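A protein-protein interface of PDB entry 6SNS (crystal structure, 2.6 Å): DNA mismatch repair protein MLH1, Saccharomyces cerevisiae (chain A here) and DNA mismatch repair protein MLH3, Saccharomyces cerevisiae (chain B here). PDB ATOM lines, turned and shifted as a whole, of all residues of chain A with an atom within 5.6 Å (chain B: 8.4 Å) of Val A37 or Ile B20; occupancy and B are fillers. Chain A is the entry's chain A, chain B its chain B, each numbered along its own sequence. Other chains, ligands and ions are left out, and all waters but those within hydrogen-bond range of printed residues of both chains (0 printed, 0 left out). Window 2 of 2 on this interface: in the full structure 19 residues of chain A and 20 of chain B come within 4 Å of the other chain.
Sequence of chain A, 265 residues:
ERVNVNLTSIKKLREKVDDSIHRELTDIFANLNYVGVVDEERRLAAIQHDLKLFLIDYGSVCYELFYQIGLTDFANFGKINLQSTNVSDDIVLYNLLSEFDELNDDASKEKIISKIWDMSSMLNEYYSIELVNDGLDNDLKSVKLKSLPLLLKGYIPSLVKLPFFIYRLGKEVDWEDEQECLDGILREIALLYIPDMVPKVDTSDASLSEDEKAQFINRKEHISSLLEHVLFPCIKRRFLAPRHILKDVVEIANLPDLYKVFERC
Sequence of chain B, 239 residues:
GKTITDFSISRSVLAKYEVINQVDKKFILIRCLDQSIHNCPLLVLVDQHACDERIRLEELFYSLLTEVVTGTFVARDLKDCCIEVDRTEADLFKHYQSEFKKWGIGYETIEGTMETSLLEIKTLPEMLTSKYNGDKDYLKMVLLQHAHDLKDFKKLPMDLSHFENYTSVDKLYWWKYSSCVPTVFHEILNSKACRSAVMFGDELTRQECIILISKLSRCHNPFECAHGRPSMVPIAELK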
ATOM      1  N   TYR A  34      -0.789  -8.921   3.509  1.00  0.00           N
ATOM      2  CA  TYR A  34       0.581  -8.971   4.014  1.00  0.00           C
ATOM      3  C   TYR A  34       0.696  -8.393   5.421  1.00  0.00           C
ATOM      4  O   TYR A  34       0.296  -7.251   5.670  1.00  0.00           O
ATOM      5  CB  TYR A  34       1.555  -8.317   3.014  1.00  0.00           C
ATOM      6  CG  TYR A  34       2.962  -8.075   3.522  1.00  0.00           C
ATOM      7  CD1 TYR A  34       3.911  -9.092   3.525  1.00  0.00           C
ATOM      8  CD2 TYR A  34       3.369  -6.806   3.923  1.00  0.00           C
ATOM      9  CE1 TYR A  34       5.214  -8.866   3.966  1.00  0.00           C
ATOM     10  CE2 TYR A  34       4.666  -6.568   4.370  1.00  0.00           C
ATOM     11  CZ  TYR A  34       5.591  -7.595   4.372  1.00  0.00           C
ATOM     12  OH  TYR A  34       6.860  -7.339   4.828  1.00  0.00           O
ATOM     13  N   VAL A  35       1.190  -9.227   6.345  1.00  0.00           N
ATOM     14  CA  VAL A  35       1.417  -8.898   7.750  1.00  0.00           C
ATOM     15  C   VAL A  35       2.847  -8.317   7.881  1.00  0.00           C
ATOM     16  O   VAL A  35       2.989  -7.131   8.214  1.00  0.00           O
ATOM     17  CB  VAL A  35       1.131 -10.118   8.682  1.00  0.00           C
ATOM     18  CG1 VAL A  35       1.466  -9.817  10.149  1.00  0.00           C
ATOM     19  CG2 VAL A  35      -0.317 -10.604   8.533  1.00  0.00           C
ATOM     20  N   GLY A  36       3.871  -9.123   7.560  1.00  0.00           N
ATOM     21  CA  GLY A  36       5.262  -8.671   7.613  1.00  0.00           C
ATOM     22  C   GLY A  36       6.350  -9.727   7.536  1.00  0.00           C
ATOM     23  O   GLY A  36       6.066 -10.924   7.561  1.00  0.00           O
ATOM     24  N   VAL A  37       7.619  -9.271   7.463  1.00  0.00           N
ATOM     25  CA  VAL A  37       8.809 -10.128   7.390  1.00  0.00           C
ATOM     26  C   VAL A  37       8.987 -10.909   8.699  1.00  0.00           C
ATOM     27  O   VAL A  37       8.986 -10.322   9.788  1.00  0.00           O
ATOM     28  CB  VAL A  37      10.097  -9.343   7.010  1.00  0.00           C
ATOM     29  CG1 VAL A  37      11.335 -10.235   7.058  1.00  0.00           C
ATOM     30  CG2 VAL A  37       9.965  -8.690   5.645  1.00  0.00           C
ATOM     31  N   VAL A  38       9.150 -12.233   8.561  1.00  0.00           N
ATOM     32  CA  VAL A  38       9.344 -13.220   9.623  1.00  0.00           C
ATOM     33  C   VAL A  38      10.829 -13.590   9.702  1.00  0.00           C
ATOM     34  O   VAL A  38      11.351 -13.743  10.802  1.00  0.00           O
ATOM     35  CB  VAL A  38       8.446 -14.452   9.345  1.00  0.00           C
ATOM     36  CG1 VAL A  38       8.800 -15.638  10.239  1.00  0.00           C
ATOM     37  CG2 VAL A  38       6.968 -14.091   9.474  1.00  0.00           C
ATOM     38  N   ASP A  39      11.507 -13.725   8.542  1.00  0.00           N
ATOM     39  CA  ASP A  39      12.923 -14.095   8.466  1.00  0.00           C
ATOM     40  C   ASP A  39      13.563 -13.485   7.231  1.00  0.00           C
ATOM     41  O   ASP A  39      13.227 -13.869   6.116  1.00  0.00           O
ATOM     42  CB  ASP A  39      13.074 -15.632   8.429  1.00  0.00           C
ATOM     43  CG  ASP A  39      14.431 -16.192   8.812  1.00  0.00           C
ATOM     44  OD1 ASP A  39      15.453 -15.527   8.534  1.00  0.00           O
ATOM     45  OD2 ASP A  39      14.473 -17.309   9.368  1.00  0.00           O
ATOM     46  N   GLU A  40      14.496 -12.545   7.433  1.00  0.00           N
ATOM     47  CA  GLU A  40      15.230 -11.860   6.364  1.00  0.00           C
ATOM     48  C   GLU A  40      16.238 -12.786   5.681  1.00  0.00           C
ATOM     49  O   GLU A  40      16.504 -12.626   4.485  1.00  0.00           O
ATOM     50  CB  GLU A  40      15.962 -10.632   6.917  1.00  0.00           C
ATOM     51  CG  GLU A  40      15.052  -9.464   7.269  1.00  0.00           C
ATOM     52  CD  GLU A  40      14.525  -9.403   8.692  1.00  0.00           C
ATOM     53  OE1 GLU A  40      13.804  -8.427   9.006  1.00  0.00           O
ATOM     54  OE2 GLU A  40      14.832 -10.318   9.493  1.00  0.00           O
ATOM     55  N   LEU A  44      11.422 -15.287   4.612  1.00  0.00           N
ATOM     56  CA  LEU A  44      10.068 -15.645   5.046  1.00  0.00           C
ATOM     57  C   LEU A  44       9.284 -14.434   5.482  1.00  0.00           C
ATOM     58  O   LEU A  44       9.817 -13.578   6.188  1.00  0.00           O
ATOM     59  CB  LEU A  44      10.085 -16.680   6.189  1.00  0.00           C
ATOM     60  CG  LEU A  44      10.753 -18.026   5.907  1.00  0.00           C
ATOM     61  CD1 LEU A  44      10.725 -18.888   7.133  1.00  0.00           C
ATOM     62  CD2 LEU A  44      10.093 -18.754   4.726  1.00  0.00           C
ATOM     63  N   ALA A  45       8.017 -14.368   5.058  1.00  0.00           N
ATOM     64  CA  ALA A  45       7.079 -13.291   5.362  1.00  0.00           C
ATOM     65  C   ALA A  45       5.768 -13.913   5.791  1.00  0.00           C
ATOM     66  O   ALA A  45       5.604 -15.124   5.657  1.00  0.00           O
ATOM     67  CB  ALA A  45       6.867 -12.426   4.135  1.00  0.00           C
ATOM     68  N   ALA A  46       4.843 -13.113   6.328  1.00  0.00           N
ATOM     69  CA  ALA A  46       3.548 -13.620   6.769  1.00  0.00           C
ATOM     70  C   ALA A  46       2.424 -12.880   6.090  1.00  0.00           C
ATOM     71  O   ALA A  46       2.476 -11.659   5.971  1.00  0.00           O
ATOM     72  CB  ALA A  46       3.417 -13.516   8.279  1.00  0.00           C
ATOM     73  N   TYR A  58       9.176 -15.604   0.272  1.00  0.00           N
ATOM     74  CA  TYR A  58       9.033 -14.532  -0.704  1.00  0.00           C
ATOM     75  C   TYR A  58      10.103 -14.578  -1.784  1.00  0.00           C
ATOM     76  O   TYR A  58       9.825 -14.137  -2.890  1.00  0.00           O
ATOM     77  CB  TYR A  58       8.901 -13.140  -0.058  1.00  0.00           C
ATOM     78  CG  TYR A  58      10.035 -12.701   0.838  1.00  0.00           C
ATOM     79  CD1 TYR A  58      11.180 -12.116   0.307  1.00  0.00           C
ATOM     80  CD2 TYR A  58       9.910 -12.744   2.220  1.00  0.00           C
ATOM     81  CE1 TYR A  58      12.196 -11.639   1.133  1.00  0.00           C
ATOM     82  CE2 TYR A  58      10.910 -12.253   3.056  1.00  0.00           C
ATOM     83  CZ  TYR A  58      12.059 -11.713   2.508  1.00  0.00           C
ATOM     84  OH  TYR A  58      13.067 -11.267   3.327  1.00  0.00           O
ATOM     85  N   ILE A 223      14.226  -4.013   3.349  1.00  0.00           N
ATOM     86  CA  ILE A 223      13.596  -5.233   2.859  1.00  0.00           C
ATOM     87  C   ILE A 223      12.096  -5.208   3.135  1.00  0.00           C
ATOM     88  O   ILE A 223      11.312  -5.503   2.232  1.00  0.00           O
ATOM     89  CB  ILE A 223      14.342  -6.476   3.420  1.00  0.00           C
ATOM     90  CG1 ILE A 223      15.665  -6.751   2.636  1.00  0.00           C
ATOM     91  CG2 ILE A 223      13.463  -7.728   3.530  1.00  0.00           C
ATOM     92  CD1 ILE A 223      15.589  -7.096   1.044  1.00  0.00           C
ATOM     93  N   SER A 224      11.699  -4.797   4.356  1.00  0.00           N
ATOM     94  CA  SER A 224      10.291  -4.708   4.738  1.00  0.00           C
ATOM     95  C   SER A 224       9.528  -3.661   3.928  1.00  0.00           C
ATOM     96  O   SER A 224       8.362  -3.893   3.596  1.00  0.00           O
ATOM     97  CB  SER A 224      10.143  -4.437   6.227  1.00  0.00           C
ATOM     98  OG  SER A 224       8.789  -4.632   6.601  1.00  0.00           O
ATOM     99  N   LEU A 227       8.976  -5.010   0.305  1.00  0.00           N
ATOM    100  CA  LEU A 227       7.966  -6.050   0.380  1.00  0.00           C
ATOM    101  C   LEU A 227       6.554  -5.508   0.550  1.00  0.00           C
ATOM    102  O   LEU A 227       5.649  -5.958  -0.145  1.00  0.00           O
ATOM    103  CB  LEU A 227       8.323  -7.017   1.510  1.00  0.00           C
ATOM    104  CG  LEU A 227       8.885  -8.353   1.085  1.00  0.00           C
ATOM    105  CD1 LEU A 227      10.319  -8.235   0.635  1.00  0.00           C
ATOM    106  CD2 LEU A 227       8.832  -9.307   2.214  1.00  0.00           C
ATOM    107  N   TYR B  17      11.673 -10.600  21.936  1.00  0.00           N
ATOM    108  CA  TYR B  17      10.667 -10.613  20.875  1.00  0.00           C
ATOM    109  C   TYR B  17      10.551  -9.300  20.136  1.00  0.00           C
ATOM    110  O   TYR B  17      10.509  -8.236  20.746  1.00  0.00           O
ATOM    111  CB  TYR B  17       9.293 -11.079  21.385  1.00  0.00           C
ATOM    112  CG  TYR B  17       9.142 -12.581  21.348  1.00  0.00           C
ATOM    113  CD1 TYR B  17       9.538 -13.367  22.425  1.00  0.00           C
ATOM    114  CD2 TYR B  17       8.663 -13.225  20.213  1.00  0.00           C
ATOM    115  CE1 TYR B  17       9.441 -14.755  22.382  1.00  0.00           C
ATOM    116  CE2 TYR B  17       8.565 -14.611  20.155  1.00  0.00           C
ATOM    117  CZ  TYR B  17       8.951 -15.375  21.245  1.00  0.00           C
ATOM    118  OH  TYR B  17       8.858 -16.746  21.191  1.00  0.00           O
ATOM    119  N   GLU B  18      10.506  -9.394  18.806  1.00  0.00           N
ATOM    120  CA  GLU B  18      10.376  -8.285  17.864  1.00  0.00           C
ATOM    121  C   GLU B  18       8.939  -8.282  17.315  1.00  0.00           C
ATOM    122  O   GLU B  18       8.378  -9.345  17.019  1.00  0.00           O
ATOM    123  CB  GLU B  18      11.407  -8.437  16.721  1.00  0.00           C
ATOM    124  CG  GLU B  18      12.143  -7.157  16.361  1.00  0.00           C
ATOM    125  CD  GLU B  18      12.109  -6.756  14.896  1.00  0.00           C
ATOM    126  OE1 GLU B  18      13.120  -6.193  14.412  1.00  0.00           O
ATOM    127  OE2 GLU B  18      11.071  -6.993  14.232  1.00  0.00           O
ATOM    128  N   VAL B  19       8.337  -7.097  17.218  1.00  0.00           N
ATOM    129  CA  VAL B  19       6.970  -6.953  16.711  1.00  0.00           C
ATOM    130  C   VAL B  19       6.986  -7.080  15.187  1.00  0.00           C
ATOM    131  O   VAL B  19       7.877  -6.542  14.542  1.00  0.00           O
ATOM    132  CB  VAL B  19       6.336  -5.607  17.171  1.00  0.00           C
ATOM    133  CG1 VAL B  19       4.913  -5.446  16.645  1.00  0.00           C
ATOM    134  CG2 VAL B  19       6.369  -5.471  18.689  1.00  0.00           C
ATOM    135  N   ILE B  20       6.031  -7.808  14.621  1.00  0.00           N
ATOM    136  CA  ILE B  20       5.906  -7.906  13.178  1.00  0.00           C
ATOM    137  C   ILE B  20       4.865  -6.849  12.807  1.00  0.00           C
ATOM    138  O   ILE B  20       5.241  -5.810  12.269  1.00  0.00           O
ATOM    139  CB  ILE B  20       5.616  -9.340  12.655  1.00  0.00           C
ATOM    140  CG1 ILE B  20       6.783 -10.294  13.016  1.00  0.00           C
ATOM    141  CG2 ILE B  20       5.332  -9.325  11.132  1.00  0.00           C
ATOM    142  CD1 ILE B  20       6.698 -11.693  12.487  1.00  0.00           C
ATOM    143  N   ASN B  21       3.584  -7.070  13.168  1.00  0.00           N
ATOM    144  CA  ASN B  21       2.470  -6.138  12.963  1.00  0.00           C
ATOM    145  C   ASN B  21       1.154  -6.734  13.508  1.00  0.00           C
ATOM    146  O   ASN B  21       1.138  -7.896  13.927  1.00  0.00           O
ATOM    147  CB  ASN B  21       2.337  -5.742  11.492  1.00  0.00           C
ATOM    148  CG  ASN B  21       1.662  -4.416  11.250  1.00  0.00           C
ATOM    149  OD1 ASN B  21       1.298  -3.661  12.181  1.00  0.00           O
ATOM    150  ND2 ASN B  21       1.459  -4.116   9.976  1.00  0.00           N
ATOM    151  N   GLN B  22       0.066  -5.924  13.529  1.00  0.00           N
ATOM    152  CA  GLN B  22      -1.278  -6.314  13.975  1.00  0.00           C
ATOM    153  C   GLN B  22      -1.927  -7.320  13.000  1.00  0.00           C
ATOM    154  O   GLN B  22      -1.804  -7.187  11.777  1.00  0.00           O
ATOM    155  CB  GLN B  22      -2.156  -5.069  14.170  1.00  0.00           C
ATOM    156  CG  GLN B  22      -3.625  -5.348  14.488  1.00  0.00           C
ATOM    157  CD  GLN B  22      -4.378  -4.085  14.811  1.00  0.00           C
ATOM    158  OE1 GLN B  22      -4.423  -3.124  14.038  1.00  0.00           O
ATOM    159  NE2 GLN B  22      -4.995  -4.065  15.970  1.00  0.00           N
ATOM    160  N   VAL B  23      -2.603  -8.334  13.555  1.00  0.00           N
ATOM    161  CA  VAL B  23      -3.255  -9.388  12.779  1.00  0.00           C
ATOM    162  C   VAL B  23      -4.750  -9.425  13.099  1.00  0.00           C
ATOM    163  O   VAL B  23      -5.116  -9.747  14.231  1.00  0.00           O
ATOM    164  CB  VAL B  23      -2.606 -10.774  13.046  1.00  0.00           C
ATOM    165  CG1 VAL B  23      -3.236 -11.844  12.172  1.00  0.00           C
ATOM    166  CG2 VAL B  23      -1.099 -10.742  12.855  1.00  0.00           C
ATOM    167  N   ILE B  28      -1.359  -9.242  17.909  1.00  0.00           N
ATOM    168  CA  ILE B  28      -0.113  -8.578  17.548  1.00  0.00           C
ATOM    169  C   ILE B  28       0.876  -9.728  17.310  1.00  0.00           C
ATOM    170  O   ILE B  28       1.204 -10.445  18.272  1.00  0.00           O
ATOM    171  CB  ILE B  28       0.366  -7.585  18.644  1.00  0.00           C
ATOM    172  CG1 ILE B  28      -0.596  -6.370  18.764  1.00  0.00           C
ATOM    173  CG2 ILE B  28       1.820  -7.138  18.389  1.00  0.00           C
ATOM    174  CD1 ILE B  28      -0.664  -5.755  20.159  1.00  0.00           C
ATOM    175  N   LEU B  29       1.292  -9.955  16.033  1.00  0.00           N
ATOM    176  CA  LEU B  29       2.231 -11.038  15.723  1.00  0.00           C
ATOM    177  C   LEU B  29       3.643 -10.631  16.062  1.00  0.00           C
ATOM    178  O   LEU B  29       4.120  -9.615  15.568  1.00  0.00           O
ATOM    179  CB  LEU B  29       2.134 -11.523  14.264  1.00  0.00           C
ATOM    180  CG  LEU B  29       2.987 -12.737  13.846  1.00  0.00           C
ATOM    181  CD1 LEU B  29       2.724 -13.971  14.719  1.00  0.00           C
ATOM    182  CD2 LEU B  29       2.743 -13.076  12.408  1.00  0.00           C
ATOM    183  N   ILE B  30       4.289 -11.417  16.933  1.00  0.00           N
ATOM    184  CA  ILE B  30       5.658 -11.191  17.387  1.00  0.00           C
ATOM    185  C   ILE B  30       6.585 -12.380  17.008  1.00  0.00           C
ATOM    186  O   ILE B  30       6.120 -13.528  16.895  1.00  0.00           O
ATOM    187  CB  ILE B  30       5.717 -10.811  18.897  1.00  0.00           C
ATOM    188  CG1 ILE B  30       5.121 -11.908  19.808  1.00  0.00           C
ATOM    189  CG2 ILE B  30       5.056  -9.448  19.148  1.00  0.00           C
ATOM    190  CD1 ILE B  30       5.605 -11.886  21.263  1.00  0.00           C
ATOM    191  N   ARG B  31       7.890 -12.086  16.797  1.00  0.00           N
ATOM    192  CA  ARG B  31       8.919 -13.066  16.407  1.00  0.00           C
ATOM    193  C   ARG B  31      10.154 -13.007  17.304  1.00  0.00           C
ATOM    194  O   ARG B  31      10.545 -11.916  17.709  1.00  0.00           O
ATOM    195  CB  ARG B  31       9.313 -12.913  14.921  1.00  0.00           C
ATOM    196  CG  ARG B  31       9.867 -11.535  14.539  1.00  0.00           C
ATOM    197  CD  ARG B  31      10.701 -11.599  13.288  1.00  0.00           C
ATOM    198  NE  ARG B  31      10.919 -10.270  12.723  1.00  0.00           N
ATOM    199  CZ  ARG B  31      11.869  -9.979  11.841  1.00  0.00           C
ATOM    200  NH1 ARG B  31      12.707 -10.919  11.421  1.00  0.00           N
ATOM    201  NH2 ARG B  31      11.999  -8.742  11.381  1.00  0.00           N
ATOM    202  N   CYS B  32      10.775 -14.171  17.597  1.00  0.00           N
ATOM    203  CA  CYS B  32      11.955 -14.277  18.467  1.00  0.00           C
ATOM    204  C   CYS B  32      13.233 -13.692  17.840  1.00  0.00           C
ATOM    205  O   CYS B  32      13.562 -13.979  16.689  1.00  0.00           O
ATOM    206  CB  CYS B  32      12.160 -15.717  18.928  1.00  0.00           C
ATOM    207  SG  CYS B  32      13.037 -15.880  20.507  1.00  0.00           S
ATOM    208  N   LEU B  42       9.152 -19.228  17.999  1.00  0.00           N
ATOM    209  CA  LEU B  42       9.556 -18.366  16.884  1.00  0.00           C
ATOM    210  C   LEU B  42       8.488 -17.328  16.575  1.00  0.00           C
ATOM    211  O   LEU B  42       8.827 -16.189  16.244  1.00  0.00           O
ATOM    212  CB  LEU B  42       9.910 -19.189  15.606  1.00  0.00           C
ATOM    213  CG  LEU B  42       9.951 -18.439  14.232  1.00  0.00           C
ATOM    214  CD1 LEU B  42      11.208 -17.580  14.075  1.00  0.00           C
ATOM    215  CD2 LEU B  42       9.802 -19.393  13.063  1.00  0.00           C
ATOM    216  N   LEU B  43       7.208 -17.741  16.620  1.00  0.00           N
ATOM    217  CA  LEU B  43       6.073 -16.849  16.364  1.00  0.00           C
ATOM    218  C   LEU B  43       5.009 -16.987  17.438  1.00  0.00           C
ATOM    219  O   LEU B  43       4.617 -18.108  17.791  1.00  0.00           O
ATOM    220  CB  LEU B  43       5.458 -17.054  14.966  1.00  0.00           C
ATOM    221  CG  LEU B  43       6.256 -16.565  13.763  1.00  0.00           C
ATOM    222  CD1 LEU B  43       5.711 -17.153  12.499  1.00  0.00           C
ATOM    223  CD2 LEU B  43       6.238 -15.065  13.656  1.00  0.00           C
ATOM    224  N   VAL B  44       4.564 -15.839  17.979  1.00  0.00           N
ATOM    225  CA  VAL B  44       3.533 -15.788  19.016  1.00  0.00           C
ATOM    226  C   VAL B  44       2.507 -14.726  18.642  1.00  0.00           C
ATOM    227  O   VAL B  44       2.878 -13.637  18.198  1.00  0.00           O
ATOM    228  CB  VAL B  44       4.110 -15.515  20.439  1.00  0.00           C
ATOM    229  CG1 VAL B  44       3.087 -15.835  21.516  1.00  0.00           C
ATOM    230  CG2 VAL B  44       5.397 -16.288  20.698  1.00  0.00           C
ATOM    231  N   LEU B  45       1.219 -15.038  18.822  1.00  0.00           N
ATOM    232  CA  LEU B  45       0.153 -14.062  18.615  1.00  0.00           C
ATOM    233  C   LEU B  45      -0.277 -13.588  20.009  1.00  0.00           C
ATOM    234  O   LEU B  45      -0.754 -14.384  20.820  1.00  0.00           O
ATOM    235  CB  LEU B  45      -1.048 -14.641  17.830  1.00  0.00           C
ATOM    236  CG  LEU B  45      -0.875 -14.832  16.319  1.00  0.00           C
ATOM    237  CD1 LEU B  45      -1.942 -15.754  15.771  1.00  0.00           C
ATOM    238  CD2 LEU B  45      -0.894 -13.496  15.566  1.00  0.00           C
ATOM    239  N   THR B 205      -1.389   0.815  15.076  1.00  0.00           N
ATOM    240  CA  THR B 205      -0.264   1.005  14.154  1.00  0.00           C
ATOM    241  C   THR B 205       0.886   0.115  14.641  1.00  0.00           C
ATOM    242  O   THR B 205       0.896  -0.253  15.814  1.00  0.00           O
ATOM    243  CB  THR B 205       0.205   2.474  14.131  1.00  0.00           C
ATOM    244  OG1 THR B 205       0.771   2.825  15.392  1.00  0.00           O
ATOM    245  CG2 THR B 205      -0.889   3.445  13.753  1.00  0.00           C
ATOM    246  N   ARG B 206       1.863  -0.208  13.775  1.00  0.00           N
ATOM    247  CA  ARG B 206       3.035  -1.005  14.158  1.00  0.00           C
ATOM    248  C   ARG B 206       3.710  -0.367  15.389  1.00  0.00           C
ATOM    249  O   ARG B 206       4.093  -1.084  16.315  1.00  0.00           O
ATOM    250  CB  ARG B 206       4.036  -1.116  12.990  1.00  0.00           C
ATOM    251  CG  ARG B 206       4.581  -2.526  12.774  1.00  0.00           C
ATOM    252  CD  ARG B 206       5.794  -2.548  11.866  1.00  0.00           C
ATOM    253  NE  ARG B 206       7.036  -2.284  12.595  1.00  0.00           N
ATOM    254  CZ  ARG B 206       7.900  -3.225  12.964  1.00  0.00           C
ATOM    255  NH1 ARG B 206       7.673  -4.497  12.666  1.00  0.00           N
ATOM    256  NH2 ARG B 206       9.009  -2.900  13.619  1.00  0.00           N
ATOM    257  N   GLN B 207       3.790   0.982  15.417  1.00  0.00           N
ATOM    258  CA  GLN B 207       4.360   1.744  16.525  1.00  0.00           C
ATOM    259  C   GLN B 207       3.590   1.495  17.817  1.00  0.00           C
ATOM    260  O   GLN B 207       4.221   1.136  18.811  1.00  0.00           O
ATOM    261  CB  GLN B 207       4.452   3.246  16.188  1.00  0.00           C
ATOM    262  CG  GLN B 207       5.028   4.132  17.307  1.00  0.00           C
ATOM    263  CD  GLN B 207       6.452   3.790  17.695  1.00  0.00           C
ATOM    264  OE1 GLN B 207       6.704   3.105  18.694  1.00  0.00           O
ATOM    265  NE2 GLN B 207       7.417   4.264  16.920  1.00  0.00           N
ATOM    266  N   CYS B 209       1.833  -1.016  18.610  1.00  0.00           N
ATOM    267  CA  CYS B 209       2.100  -2.414  18.971  1.00  0.00           C
ATOM    268  C   CYS B 209       3.483  -2.545  19.606  1.00  0.00           C
ATOM    269  O   CYS B 209       3.624  -3.231  20.614  1.00  0.00           O
ATOM    270  CB  CYS B 209       1.952  -3.342  17.767  1.00  0.00           C
ATOM    271  SG  CYS B 209       0.349  -3.238  16.929  1.00  0.00           S
ATOM    272  N   ILE B 210       4.497  -1.883  19.030  1.00  0.00           N
ATOM    273  CA  ILE B 210       5.843  -1.914  19.592  1.00  0.00           C
ATOM    274  C   ILE B 210       5.767  -1.489  21.049  1.00  0.00           C
ATOM    275  O   ILE B 210       6.276  -2.209  21.902  1.00  0.00           O
ATOM    276  CB  ILE B 210       6.868  -1.106  18.739  1.00  0.00           C
ATOM    277  CG1 ILE B 210       7.342  -1.954  17.531  1.00  0.00           C
ATOM    278  CG2 ILE B 210       8.080  -0.637  19.571  1.00  0.00           C
ATOM    279  CD1 ILE B 210       7.615  -1.169  16.255  1.00  0.00           C
ATOM    280  N   ILE B 213       3.805  -4.137  23.476  1.00  0.00           N
ATOM    281  CA  ILE B 213       4.639  -5.293  23.758  1.00  0.00           C
ATOM    282  C   ILE B 213       5.864  -4.890  24.566  1.00  0.00           C
ATOM    283  O   ILE B 213       6.326  -5.670  25.404  1.00  0.00           O
ATOM    284  CB  ILE B 213       4.946  -6.065  22.465  1.00  0.00           C
ATOM    285  CG1 ILE B 213       3.677  -6.250  21.574  1.00  0.00           C
ATOM    286  CG2 ILE B 213       5.653  -7.391  22.742  1.00  0.00           C
ATOM    287  CD1 ILE B 213       2.480  -7.061  22.126  1.00  0.00           C
ATOM    288  N   ILE B 235       2.383 -19.823  17.998  1.00  0.00           N
ATOM    289  CA  ILE B 235       1.844 -20.542  16.837  1.00  0.00           C
ATOM    290  C   ILE B 235       2.890 -21.472  16.175  1.00  0.00           C
ATOM    291  O   ILE B 235       2.504 -22.500  15.599  1.00  0.00           O
ATOM    292  CB  ILE B 235       1.139 -19.598  15.816  1.00  0.00           C
ATOM    293  CG1 ILE B 235       2.034 -18.407  15.395  1.00  0.00           C
ATOM    294  CG2 ILE B 235      -0.213 -19.126  16.379  1.00  0.00           C
ATOM    295  CD1 ILE B 235       1.520 -17.596  14.240  1.00  0.00           C
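The side-chain carboxylate of Glu A40 lies within salt-bridge range of the guanidinium group of Arg B31, at 2.9 Å.
O of Val A38 sits at hydrogen-bond distance from NH1 of Arg B31 (3.2 Å).
Val A37 touches just these residues of chain B: Ile B20 and Arg B31.
Of the printed residues of chain A, Ile B20 touches Gly A36, Val A37 and Val A38.
Of the printed residues of chain B, Val A38 touches Ile B20 (3.9 Å) and Arg B31 (3.2 Å).
Of the printed residues of chain A, Asn B21 touches Val A35 (3.6 Å).
Tyr B17 touches none of the printed residues of chain A.
Ile B213 touches none of the printed residues of chain A.
The nearest residue of chain B that does not touch Val A37 is Glu B18 (5.9 Å).
The nearest printed residue of chain B that does not touch Val A35 is Ile B20 (4.02 Å).
Val A35 touches Asn B21 (O to CB, 3.6 Å).
CG1 of Val A35 touches CG2 of Val B23 (3.8 Å).
Ile B20 touches Gly A36 (CG2 to CA, 3.6 Å).
Val A37 touches Ile B20 (O to CD1, 3.8 Å).
Val A37 touches Arg B31 (O to NE, 3.5 Å).
Val A38 touches Ile B20 (CG2 to CD1, 3.9 Å).
The backbone NH (N) of Leu B29 lies within hydrogen-bond range of the backbone carbonyl oxygen (O) of Asn B21, 2.9 Å away.
N of Val A38 sits at hydrogen-bond distance from O of Leu A44 (2.8 Å).
O of Gly A36 is in hydrogen-bond range of N of Ala A46.
O of Leu B29 is in hydrogen-bond range of N of Ile B20, at 2.8 Å.
The backbone carbonyl oxygen (O) of Ala A46 sits at hydrogen-bond distance from the backbone NH (N) of Val A35.
O of Ile B20 is in hydrogen-bond range of NH1 of Arg B206 (2.8 Å).
Hydrophobic or aromatic side chains of chain B within 4 Å of the printed part of chain A: Ile B20 and Val B23.
Among the printed residues, Asp or Glu carboxylates within 4 Å of a Lys or Arg side-chain nitrogen of the other chain: Glu A40 with Arg B31.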
